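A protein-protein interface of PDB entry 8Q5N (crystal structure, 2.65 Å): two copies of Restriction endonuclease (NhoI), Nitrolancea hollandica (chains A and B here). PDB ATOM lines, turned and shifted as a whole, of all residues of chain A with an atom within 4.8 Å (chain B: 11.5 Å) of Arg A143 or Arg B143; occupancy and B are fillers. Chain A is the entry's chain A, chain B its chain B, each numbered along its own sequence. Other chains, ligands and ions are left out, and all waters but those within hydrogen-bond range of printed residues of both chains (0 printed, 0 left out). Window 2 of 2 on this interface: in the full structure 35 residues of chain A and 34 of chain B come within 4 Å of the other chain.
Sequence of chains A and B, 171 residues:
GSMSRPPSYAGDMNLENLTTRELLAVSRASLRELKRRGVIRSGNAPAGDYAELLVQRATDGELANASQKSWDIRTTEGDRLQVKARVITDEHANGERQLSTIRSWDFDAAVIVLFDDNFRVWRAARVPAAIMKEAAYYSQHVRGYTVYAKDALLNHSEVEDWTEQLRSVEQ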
ATOM      1  N   ARG A 103       6.309 -32.921 -17.706  1.00  0.00           N
ATOM      2  CA  ARG A 103       7.519 -32.208 -18.095  1.00  0.00           C
ATOM      3  C   ARG A 103       8.022 -32.602 -19.473  1.00  0.00           C
ATOM      4  O   ARG A 103       9.076 -32.112 -19.894  1.00  0.00           O
ATOM      5  CB  ARG A 103       8.640 -32.440 -17.068  1.00  0.00           C
ATOM      6  CG  ARG A 103       8.496 -31.686 -15.754  1.00  0.00           C
ATOM      7  CD  ARG A 103       9.481 -32.191 -14.710  1.00  0.00           C
ATOM      8  NE  ARG A 103       9.484 -31.371 -13.502  1.00  0.00           N
ATOM      9  CZ  ARG A 103       9.005 -31.746 -12.322  1.00  0.00           C
ATOM     10  NH1 ARG A 103       8.424 -32.922 -12.152  1.00  0.00           N
ATOM     11  NH2 ARG A 103       9.124 -30.920 -11.285  1.00  0.00           N
ATOM     12  N   TYR A 138       1.309 -24.112 -18.300  1.00  0.00           N
ATOM     13  CA  TYR A 138       2.716 -24.072 -17.910  1.00  0.00           C
ATOM     14  C   TYR A 138       2.901 -23.418 -16.546  1.00  0.00           C
ATOM     15  O   TYR A 138       2.201 -22.465 -16.194  1.00  0.00           O
ATOM     16  CB  TYR A 138       3.557 -23.327 -18.945  1.00  0.00           C
ATOM     17  CG  TYR A 138       5.039 -23.462 -18.672  1.00  0.00           C
ATOM     18  CD1 TYR A 138       5.657 -24.704 -18.694  1.00  0.00           C
ATOM     19  CD2 TYR A 138       5.815 -22.350 -18.360  1.00  0.00           C
ATOM     20  CE1 TYR A 138       7.007 -24.836 -18.428  1.00  0.00           C
ATOM     21  CE2 TYR A 138       7.168 -22.471 -18.095  1.00  0.00           C
ATOM     22  CZ  TYR A 138       7.756 -23.716 -18.130  1.00  0.00           C
ATOM     23  OH  TYR A 138       9.099 -23.850 -17.869  1.00  0.00           O
ATOM     24  N   SER A 139       3.857 -23.942 -15.776  1.00  0.00           N
ATOM     25  CA  SER A 139       4.256 -23.375 -14.495  1.00  0.00           C
ATOM     26  C   SER A 139       5.771 -23.243 -14.433  1.00  0.00           C
ATOM     27  O   SER A 139       6.496 -24.205 -14.712  1.00  0.00           O
ATOM     28  CB  SER A 139       3.765 -24.227 -13.323  1.00  0.00           C
ATOM     29  OG  SER A 139       4.419 -23.844 -12.125  1.00  0.00           O
ATOM     30  N   GLN A 140       6.245 -22.050 -14.072  1.00  0.00           N
ATOM     31  CA  GLN A 140       7.680 -21.815 -13.964  1.00  0.00           C
ATOM     32  C   GLN A 140       8.234 -22.371 -12.657  1.00  0.00           C
ATOM     33  O   GLN A 140       9.423 -22.703 -12.585  1.00  0.00           O
ATOM     34  CB  GLN A 140       8.004 -20.326 -14.113  1.00  0.00           C
ATOM     35  CG  GLN A 140       7.580 -19.749 -15.463  1.00  0.00           C
ATOM     36  CD  GLN A 140       7.904 -18.275 -15.609  1.00  0.00           C
ATOM     37  N   HIS A 141       7.401 -22.463 -11.615  1.00  0.00           N
ATOM     38  CA  HIS A 141       7.877 -22.979 -10.335  1.00  0.00           C
ATOM     39  C   HIS A 141       8.295 -24.440 -10.445  1.00  0.00           C
ATOM     40  O   HIS A 141       9.213 -24.884  -9.749  1.00  0.00           O
ATOM     41  CB  HIS A 141       6.777 -22.871  -9.275  1.00  0.00           C
ATOM     42  CG  HIS A 141       6.476 -21.477  -8.822  1.00  0.00           C
ATOM     43  ND1 HIS A 141       5.214 -20.930  -8.901  1.00  0.00           N
ATOM     44  CD2 HIS A 141       7.260 -20.536  -8.245  1.00  0.00           C
ATOM     45  CE1 HIS A 141       5.240 -19.702  -8.415  1.00  0.00           C
ATOM     46  NE2 HIS A 141       6.469 -19.439  -8.010  1.00  0.00           N
ATOM     47  N   VAL A 142       7.626 -25.205 -11.304  1.00  0.00           N
ATOM     48  CA  VAL A 142       7.865 -26.640 -11.412  1.00  0.00           C
ATOM     49  C   VAL A 142       8.567 -27.063 -12.695  1.00  0.00           C
ATOM     50  O   VAL A 142       8.966 -28.237 -12.794  1.00  0.00           O
ATOM     51  CB  VAL A 142       6.553 -27.436 -11.245  1.00  0.00           C
ATOM     52  CG1 VAL A 142       5.881 -27.076  -9.927  1.00  0.00           C
ATOM     53  CG2 VAL A 142       5.622 -27.146 -12.398  1.00  0.00           C
ATOM     54  N   ARG A 143       8.711 -26.176 -13.687  1.00  0.00           N
ATOM     55  CA  ARG A 143       9.307 -26.545 -14.977  1.00  0.00           C
ATOM     56  C   ARG A 143       8.481 -27.630 -15.664  1.00  0.00           C
ATOM     57  O   ARG A 143       9.008 -28.632 -16.145  1.00  0.00           O
ATOM     58  CB  ARG A 143      10.768 -26.993 -14.834  1.00  0.00           C
ATOM     59  CG  ARG A 143      11.845 -25.960 -15.125  1.00  0.00           C
ATOM     60  CD  ARG A 143      11.616 -24.584 -14.536  1.00  0.00           C
ATOM     61  NE  ARG A 143      12.655 -23.684 -15.027  1.00  0.00           N
ATOM     62  CZ  ARG A 143      12.890 -22.463 -14.571  1.00  0.00           C
ATOM     63  NH1 ARG A 143      12.148 -21.925 -13.616  1.00  0.00           N
ATOM     64  NH2 ARG A 143      13.893 -21.760 -15.090  1.00  0.00           N
ATOM     65  N   GLY A 144       7.176 -27.420 -15.712  1.00  0.00           N
ATOM     66  CA  GLY A 144       6.307 -28.389 -16.337  1.00  0.00           C
ATOM     67  C   GLY A 144       4.929 -27.831 -16.585  1.00  0.00           C
ATOM     68  O   GLY A 144       4.714 -26.621 -16.521  1.00  0.00           O
ATOM     69  N   TYR A 145       3.991 -28.734 -16.862  1.00  0.00           N
ATOM     70  CA  TYR A 145       2.629 -28.371 -17.233  1.00  0.00           C
ATOM     71  C   TYR A 145       1.638 -29.061 -16.309  1.00  0.00           C
ATOM     72  O   TYR A 145       1.877 -30.186 -15.858  1.00  0.00           O
ATOM     73  CB  TYR A 145       2.325 -28.716 -18.689  1.00  0.00           C
ATOM     74  CG  TYR A 145       3.314 -28.136 -19.666  1.00  0.00           C
ATOM     75  CD1 TYR A 145       4.576 -28.699 -19.821  1.00  0.00           C
ATOM     76  CD2 TYR A 145       3.002 -27.007 -20.416  1.00  0.00           C
ATOM     77  CE1 TYR A 145       5.491 -28.164 -20.703  1.00  0.00           C
ATOM     78  CE2 TYR A 145       3.915 -26.468 -21.306  1.00  0.00           C
ATOM     79  CZ  TYR A 145       5.157 -27.055 -21.443  1.00  0.00           C
ATOM     80  OH  TYR A 145       6.084 -26.540 -22.320  1.00  0.00           O
ATOM     81  N   LYS B  69       2.929 -22.169  -4.295  1.00  0.00           N
ATOM     82  CA  LYS B  69       3.896 -23.221  -4.577  1.00  0.00           C
ATOM     83  C   LYS B  69       5.224 -22.982  -3.880  1.00  0.00           C
ATOM     84  O   LYS B  69       6.071 -23.884  -3.855  1.00  0.00           O
ATOM     85  CB  LYS B  69       4.153 -23.330  -6.089  1.00  0.00           C
ATOM     86  CG  LYS B  69       2.927 -23.279  -6.994  1.00  0.00           C
ATOM     87  CD  LYS B  69       3.294 -23.768  -8.396  1.00  0.00           C
ATOM     88  CE  LYS B  69       2.291 -23.343  -9.466  1.00  0.00           C
ATOM     89  NZ  LYS B  69       0.898 -23.217  -8.966  1.00  0.00           N
ATOM     90  N   SER B  70       5.418 -21.793  -3.323  1.00  0.00           N
ATOM     91  CA  SER B  70       6.700 -21.425  -2.748  1.00  0.00           C
ATOM     92  C   SER B  70       6.892 -21.977  -1.343  1.00  0.00           C
ATOM     93  O   SER B  70       8.038 -22.164  -0.917  1.00  0.00           O
ATOM     94  CB  SER B  70       6.834 -19.900  -2.738  1.00  0.00           C
ATOM     95  OG  SER B  70       6.590 -19.371  -4.032  1.00  0.00           O
ATOM     96  N   GLN B  98      19.850 -36.131  -0.272  1.00  0.00           N
ATOM     97  CA  GLN B  98      19.482 -35.224  -1.348  1.00  0.00           C
ATOM     98  C   GLN B  98      18.020 -34.815  -1.225  1.00  0.00           C
ATOM     99  O   GLN B  98      17.140 -35.665  -1.053  1.00  0.00           O
ATOM    100  CB  GLN B  98      19.733 -35.872  -2.707  1.00  0.00           C
ATOM    101  CG  GLN B  98      19.439 -34.947  -3.871  1.00  0.00           C
ATOM    102  CD  GLN B  98      19.664 -35.607  -5.211  1.00  0.00           C
ATOM    103  OE1 GLN B  98      20.212 -36.708  -5.295  1.00  0.00           O
ATOM    104  NE2 GLN B  98      19.272 -34.918  -6.277  1.00  0.00           N
ATOM    105  N   SER B 100      14.573 -32.572  -2.706  1.00  0.00           N
ATOM    106  CA  SER B 100      13.940 -32.223  -3.968  1.00  0.00           C
ATOM    107  C   SER B 100      14.325 -30.810  -4.399  1.00  0.00           C
ATOM    108  O   SER B 100      14.787 -29.987  -3.602  1.00  0.00           O
ATOM    109  CB  SER B 100      12.421 -32.335  -3.858  1.00  0.00           C
ATOM    110  OG  SER B 100      11.867 -31.163  -3.294  1.00  0.00           O
ATOM    111  N   THR B 101      14.093 -30.527  -5.680  1.00  0.00           N
ATOM    112  CA  THR B 101      14.572 -29.296  -6.293  1.00  0.00           C
ATOM    113  C   THR B 101      13.812 -28.086  -5.759  1.00  0.00           C
ATOM    114  O   THR B 101      12.580 -28.097  -5.680  1.00  0.00           O
ATOM    115  CB  THR B 101      14.420 -29.380  -7.812  1.00  0.00           C
ATOM    116  OG1 THR B 101      14.773 -30.697  -8.254  1.00  0.00           O
ATOM    117  CG2 THR B 101      15.315 -28.361  -8.497  1.00  0.00           C
ATOM    118  N   ILE B 102      14.551 -27.038  -5.403  1.00  0.00           N
ATOM    119  CA  ILE B 102      13.977 -25.740  -5.064  1.00  0.00           C
ATOM    120  C   ILE B 102      14.058 -24.832  -6.283  1.00  0.00           C
ATOM    121  O   ILE B 102      15.132 -24.665  -6.873  1.00  0.00           O
ATOM    122  CB  ILE B 102      14.699 -25.106  -3.863  1.00  0.00           C
ATOM    123  CG1 ILE B 102      14.594 -26.006  -2.628  1.00  0.00           C
ATOM    124  CG2 ILE B 102      14.151 -23.713  -3.573  1.00  0.00           C
ATOM    125  CD1 ILE B 102      15.480 -25.565  -1.482  1.00  0.00           C
ATOM    126  N   ARG B 103      12.919 -24.257  -6.671  1.00  0.00           N
ATOM    127  CA  ARG B 103      12.844 -23.332  -7.798  1.00  0.00           C
ATOM    128  C   ARG B 103      12.241 -21.997  -7.386  1.00  0.00           C
ATOM    129  O   ARG B 103      11.928 -21.172  -8.252  1.00  0.00           O
ATOM    130  CB  ARG B 103      12.065 -23.962  -8.958  1.00  0.00           C
ATOM    131  CG  ARG B 103      12.836 -25.095  -9.624  1.00  0.00           C
ATOM    132  CD  ARG B 103      11.985 -25.916 -10.575  1.00  0.00           C
ATOM    133  NE  ARG B 103      12.761 -26.983 -11.193  1.00  0.00           N
ATOM    134  CZ  ARG B 103      12.588 -28.270 -10.922  1.00  0.00           C
ATOM    135  NH1 ARG B 103      11.691 -28.674 -10.038  1.00  0.00           N
ATOM    136  NH2 ARG B 103      13.356 -29.172 -11.528  1.00  0.00           N
ATOM    137  N   SER B 104      12.045 -21.777  -6.089  1.00  0.00           N
ATOM    138  CA  SER B 104      11.528 -20.512  -5.594  1.00  0.00           C
ATOM    139  C   SER B 104      12.144 -20.236  -4.233  1.00  0.00           C
ATOM    140  O   SER B 104      12.178 -21.115  -3.368  1.00  0.00           O
ATOM    141  CB  SER B 104      10.000 -20.532  -5.483  1.00  0.00           C
ATOM    142  OG  SER B 104       9.528 -19.416  -4.749  1.00  0.00           O
ATOM    143  N   TRP B 105      12.602 -19.000  -4.040  1.00  0.00           N
ATOM    144  CA  TRP B 105      13.191 -18.583  -2.776  1.00  0.00           C
ATOM    145  C   TRP B 105      12.252 -17.672  -1.999  1.00  0.00           C
ATOM    146  O   TRP B 105      12.702 -16.890  -1.157  1.00  0.00           O
ATOM    147  CB  TRP B 105      14.539 -17.900  -3.018  1.00  0.00           C
ATOM    148  CG  TRP B 105      15.612 -18.848  -3.492  1.00  0.00           C
ATOM    149  CD1 TRP B 105      16.166 -18.907  -4.740  1.00  0.00           C
ATOM    150  CD2 TRP B 105      16.244 -19.882  -2.726  1.00  0.00           C
ATOM    151  NE1 TRP B 105      17.107 -19.907  -4.795  1.00  0.00           N
ATOM    152  CE2 TRP B 105      17.174 -20.521  -3.571  1.00  0.00           C
ATOM    153  CE3 TRP B 105      16.116 -20.327  -1.407  1.00  0.00           C
ATOM    154  CZ2 TRP B 105      17.970 -21.579  -3.140  1.00  0.00           C
ATOM    155  CZ3 TRP B 105      16.908 -21.379  -0.981  1.00  0.00           C
ATOM    156  CH2 TRP B 105      17.820 -21.994  -1.846  1.00  0.00           C
ATOM    157  N   ALA B 136      22.748 -24.328  -1.269  1.00  0.00           N
ATOM    158  CA  ALA B 136      22.249 -24.887  -2.511  1.00  0.00           C
ATOM    159  C   ALA B 136      23.242 -24.586  -3.627  1.00  0.00           C
ATOM    160  O   ALA B 136      24.079 -23.687  -3.518  1.00  0.00           O
ATOM    161  CB  ALA B 136      20.877 -24.313  -2.858  1.00  0.00           C
ATOM    162  N   TYR B 137      23.139 -25.346  -4.711  1.00  0.00           N
ATOM    163  CA  TYR B 137      23.885 -25.047  -5.926  1.00  0.00           C
ATOM    164  C   TYR B 137      22.946 -25.170  -7.115  1.00  0.00           C
ATOM    165  O   TYR B 137      22.169 -26.128  -7.203  1.00  0.00           O
ATOM    166  CB  TYR B 137      25.125 -25.939  -6.082  1.00  0.00           C
ATOM    167  CG  TYR B 137      24.876 -27.386  -6.431  1.00  0.00           C
ATOM    168  CD1 TYR B 137      24.623 -28.327  -5.443  1.00  0.00           C
ATOM    169  CD2 TYR B 137      24.940 -27.820  -7.747  1.00  0.00           C
ATOM    170  CE1 TYR B 137      24.414 -29.655  -5.759  1.00  0.00           C
ATOM    171  CE2 TYR B 137      24.732 -29.143  -8.070  1.00  0.00           C
ATOM    172  CZ  TYR B 137      24.470 -30.057  -7.075  1.00  0.00           C
ATOM    173  OH  TYR B 137      24.262 -31.379  -7.398  1.00  0.00           O
ATOM    174  N   TYR B 138      23.000 -24.183  -8.007  1.00  0.00           N
ATOM    175  CA  TYR B 138      22.161 -24.195  -9.197  1.00  0.00           C
ATOM    176  C   TYR B 138      22.540 -25.379 -10.081  1.00  0.00           C
ATOM    177  O   TYR B 138      23.708 -25.775 -10.155  1.00  0.00           O
ATOM    178  CB  TYR B 138      22.324 -22.874  -9.960  1.00  0.00           C
ATOM    179  CG  TYR B 138      21.270 -22.572 -11.018  1.00  0.00           C
ATOM    180  CD1 TYR B 138      21.131 -23.360 -12.157  1.00  0.00           C
ATOM    181  CD2 TYR B 138      20.439 -21.465 -10.890  1.00  0.00           C
ATOM    182  CE1 TYR B 138      20.173 -23.075 -13.116  1.00  0.00           C
ATOM    183  CE2 TYR B 138      19.482 -21.167 -11.848  1.00  0.00           C
ATOM    184  CZ  TYR B 138      19.354 -21.974 -12.958  1.00  0.00           C
ATOM    185  OH  TYR B 138      18.403 -21.678 -13.908  1.00  0.00           O
ATOM    186  N   SER B 139      21.538 -25.956 -10.737  1.00  0.00           N
ATOM    187  CA  SER B 139      21.731 -27.043 -11.687  1.00  0.00           C
ATOM    188  C   SER B 139      21.058 -26.663 -12.996  1.00  0.00           C
ATOM    189  O   SER B 139      19.870 -26.323 -13.010  1.00  0.00           O
ATOM    190  CB  SER B 139      21.157 -28.347 -11.135  1.00  0.00           C
ATOM    191  OG  SER B 139      21.043 -29.327 -12.147  1.00  0.00           O
ATOM    192  N   GLN B 140      21.811 -26.740 -14.100  1.00  0.00           N
ATOM    193  CA  GLN B 140      21.303 -26.239 -15.372  1.00  0.00           C
ATOM    194  C   GLN B 140      20.352 -27.204 -16.069  1.00  0.00           C
ATOM    195  O   GLN B 140      19.367 -26.765 -16.673  1.00  0.00           O
ATOM    196  N   HIS B 141      20.610 -28.513 -16.006  1.00  0.00           N
ATOM    197  CA  HIS B 141      19.702 -29.428 -16.692  1.00  0.00           C
ATOM    198  C   HIS B 141      18.342 -29.511 -16.008  1.00  0.00           C
ATOM    199  O   HIS B 141      17.356 -29.844 -16.674  1.00  0.00           O
ATOM    200  CB  HIS B 141      20.334 -30.811 -16.909  1.00  0.00           C
ATOM    201  CG  HIS B 141      20.733 -31.532 -15.661  1.00  0.00           C
ATOM    202  ND1 HIS B 141      21.492 -30.953 -14.666  1.00  0.00           N
ATOM    203  CD2 HIS B 141      20.529 -32.815 -15.282  1.00  0.00           C
ATOM    204  CE1 HIS B 141      21.709 -31.841 -13.712  1.00  0.00           C
ATOM    205  NE2 HIS B 141      21.136 -32.979 -14.062  1.00  0.00           N
ATOM    206  N   VAL B 142      18.259 -29.227 -14.704  1.00  0.00           N
ATOM    207  CA  VAL B 142      16.975 -29.269 -14.004  1.00  0.00           C
ATOM    208  C   VAL B 142      16.404 -27.874 -13.814  1.00  0.00           C
ATOM    209  O   VAL B 142      15.238 -27.743 -13.406  1.00  0.00           O
ATOM    210  CB  VAL B 142      17.072 -29.969 -12.631  1.00  0.00           C
ATOM    211  CG1 VAL B 142      17.699 -31.343 -12.772  1.00  0.00           C
ATOM    212  CG2 VAL B 142      17.811 -29.099 -11.633  1.00  0.00           C
ATOM    213  N   ARG B 143      17.195 -26.832 -14.072  1.00  0.00           N
ATOM    214  CA  ARG B 143      16.738 -25.446 -14.008  1.00  0.00           C
ATOM    215  C   ARG B 143      16.268 -25.080 -12.599  1.00  0.00           C
ATOM    216  O   ARG B 143      15.202 -24.488 -12.408  1.00  0.00           O
ATOM    217  N   GLY B 144      17.085 -25.420 -11.611  1.00  0.00           N
ATOM    218  CA  GLY B 144      16.732 -25.155 -10.232  1.00  0.00           C
ATOM    219  C   GLY B 144      17.916 -25.330  -9.309  1.00  0.00           C
ATOM    220  O   GLY B 144      19.069 -25.337  -9.745  1.00  0.00           O
ATOM    221  N   TYR B 145      17.617 -25.468  -8.016  1.00  0.00           N
ATOM    222  CA  TYR B 145      18.653 -25.561  -6.997  1.00  0.00           C
ATOM    223  C   TYR B 145      18.472 -26.843  -6.198  1.00  0.00           C
ATOM    224  O   TYR B 145      17.345 -27.230  -5.870  1.00  0.00           O
ATOM    225  CB  TYR B 145      18.624 -24.353  -6.037  1.00  0.00           C
ATOM    226  CG  TYR B 145      18.675 -23.009  -6.727  1.00  0.00           C
ATOM    227  CD1 TYR B 145      17.556 -22.489  -7.369  1.00  0.00           C
ATOM    228  CD2 TYR B 145      19.845 -22.261  -6.744  1.00  0.00           C
ATOM    229  CE1 TYR B 145      17.599 -21.260  -8.002  1.00  0.00           C
ATOM    230  CE2 TYR B 145      19.898 -21.033  -7.376  1.00  0.00           C
ATOM    231  CZ  TYR B 145      18.773 -20.538  -8.003  1.00  0.00           C
ATOM    232  OH  TYR B 145      18.818 -19.317  -8.636  1.00  0.00           O
ATOM    233  N   THR B 146      19.590 -27.489  -5.881  1.00  0.00           N
ATOM    234  CA  THR B 146      19.603 -28.739  -5.138  1.00  0.00           C
ATOM    235  C   THR B 146      20.307 -28.544  -3.802  1.00  0.00           C
ATOM    236  O   THR B 146      21.390 -27.956  -3.743  1.00  0.00           O
ATOM    237  CB  THR B 146      20.303 -29.839  -5.935  1.00  0.00           C
ATOM    238  OG1 THR B 146      19.580 -30.087  -7.150  1.00  0.00           O
ATOM    239  CG2 THR B 146      20.377 -31.137  -5.121  1.00  0.00           C
ATOM    240  N   VAL B 147      19.696 -29.052  -2.735  1.00  0.00           N
ATOM    241  CA  VAL B 147      20.247 -28.956  -1.390  1.00  0.00           C
ATOM    242  C   VAL B 147      20.419 -30.364  -0.847  1.00  0.00           C
ATOM    243  O   VAL B 147      19.503 -31.188  -0.944  1.00  0.00           O
ATOM    244  CB  VAL B 147      19.348 -28.117  -0.461  1.00  0.00           C
ATOM    245  CG1 VAL B 147      20.014 -27.927   0.892  1.00  0.00           C
ATOM    246  CG2 VAL B 147      19.031 -26.774  -1.090  1.00  0.00           C
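O of Val A142 sits at hydrogen-bond distance from NH2 of Arg A103, 3.1 Å away. The side-chain hydroxyl (OG) of Ser A139 lies within hydrogen-bond range of the backbone NH (N) of His A141. The backbone NH (N) of Ser A139 sits at hydrogen-bond distance from the backbone carbonyl oxygen (O) of Gly A144 (2.9 Å). NH1 of Arg A143 lies within hydrogen-bond range of O of Gln A140 (3.0 Å). The side-chain hydroxyl (OG) of Ser B70 is in hydrogen-bond range of the side-chain hydroxyl (OG) of Ser B104 (3.0 Å). The guanidinium group of Arg B103 sits at hydrogen-bond distance from the backbone carbonyl oxygen of Val B142, 3.0 Å away.
NH1 of Arg B103 touches NH2 of Arg A103, at 3.6 Å. OG of Ser A139 touches CE of Lys B69, 3.4 Å away. CD of Lys B69 touches ND1 of His A141, at 3.5 Å. Ser B70 touches His A141. Arg B103 touches His A141. His A141 touches Ser B104 (CD2 to CB, 3.9 Å). Val A142 touches Arg B103. NE of Arg A143 touches O of Arg B143, 3.7 Å away.
Of chain B, only Arg B143 (3.7 Å) comes within 4 Å of Arg A143. Of chain A, only Arg A143 comes within 4 Å of Arg B143. Printed residues of chain B within 4 Å of Ser A139: Lys B69 (3.4 Å). No residue of chain B comes within 4 Å of Gln A140. No residue of chain B comes within 4 Å of Gly A144. Printed residues of chain A within 4 Å of Arg B103: Arg A103 (3.6 Å), His A141 (3.1 Å) and Val A142 (3.9 Å). Printed residues of chain A within 4 Å of Lys B69: Ser A139 and His A141. Val B147 touches none of the printed residues of chain A. Gly B144 touches none of the printed residues of chain A. The nearest printed residue of chain A that does not touch Arg B143 is Gln A140 (6.1 Å).
Of the 21 printed residues of chain B, 5 touch a printed residue of chain A. Of the 9 printed residues of chain A, 5 touch a printed residue of chain B. Hydrophobic or aromatic side chains of chain A that line the printed part of chain B: His A141. Among the printed residues, 8 pairs touch across the chains. Among the printed residues, no Asp or Glu carboxylate lies within 4 Å of a Lys or Arg side-chain nitrogen of the other chain.
Arg A103 touches its own counterpart, Arg B103. His A141 touches Arg B103, but with the chains exchanged Arg A103 does not touch His B141 (8.4 Å). Val A142 touches Arg B103, but with the chains exchanged Arg A103 does not touch Val B142 (6.8 Å). Arg B143 touches its own counterpart, Arg A143. Of the 8 pairs that touch across the chains among the printed residues, 2 have their exchanged pair printed and touching as well.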
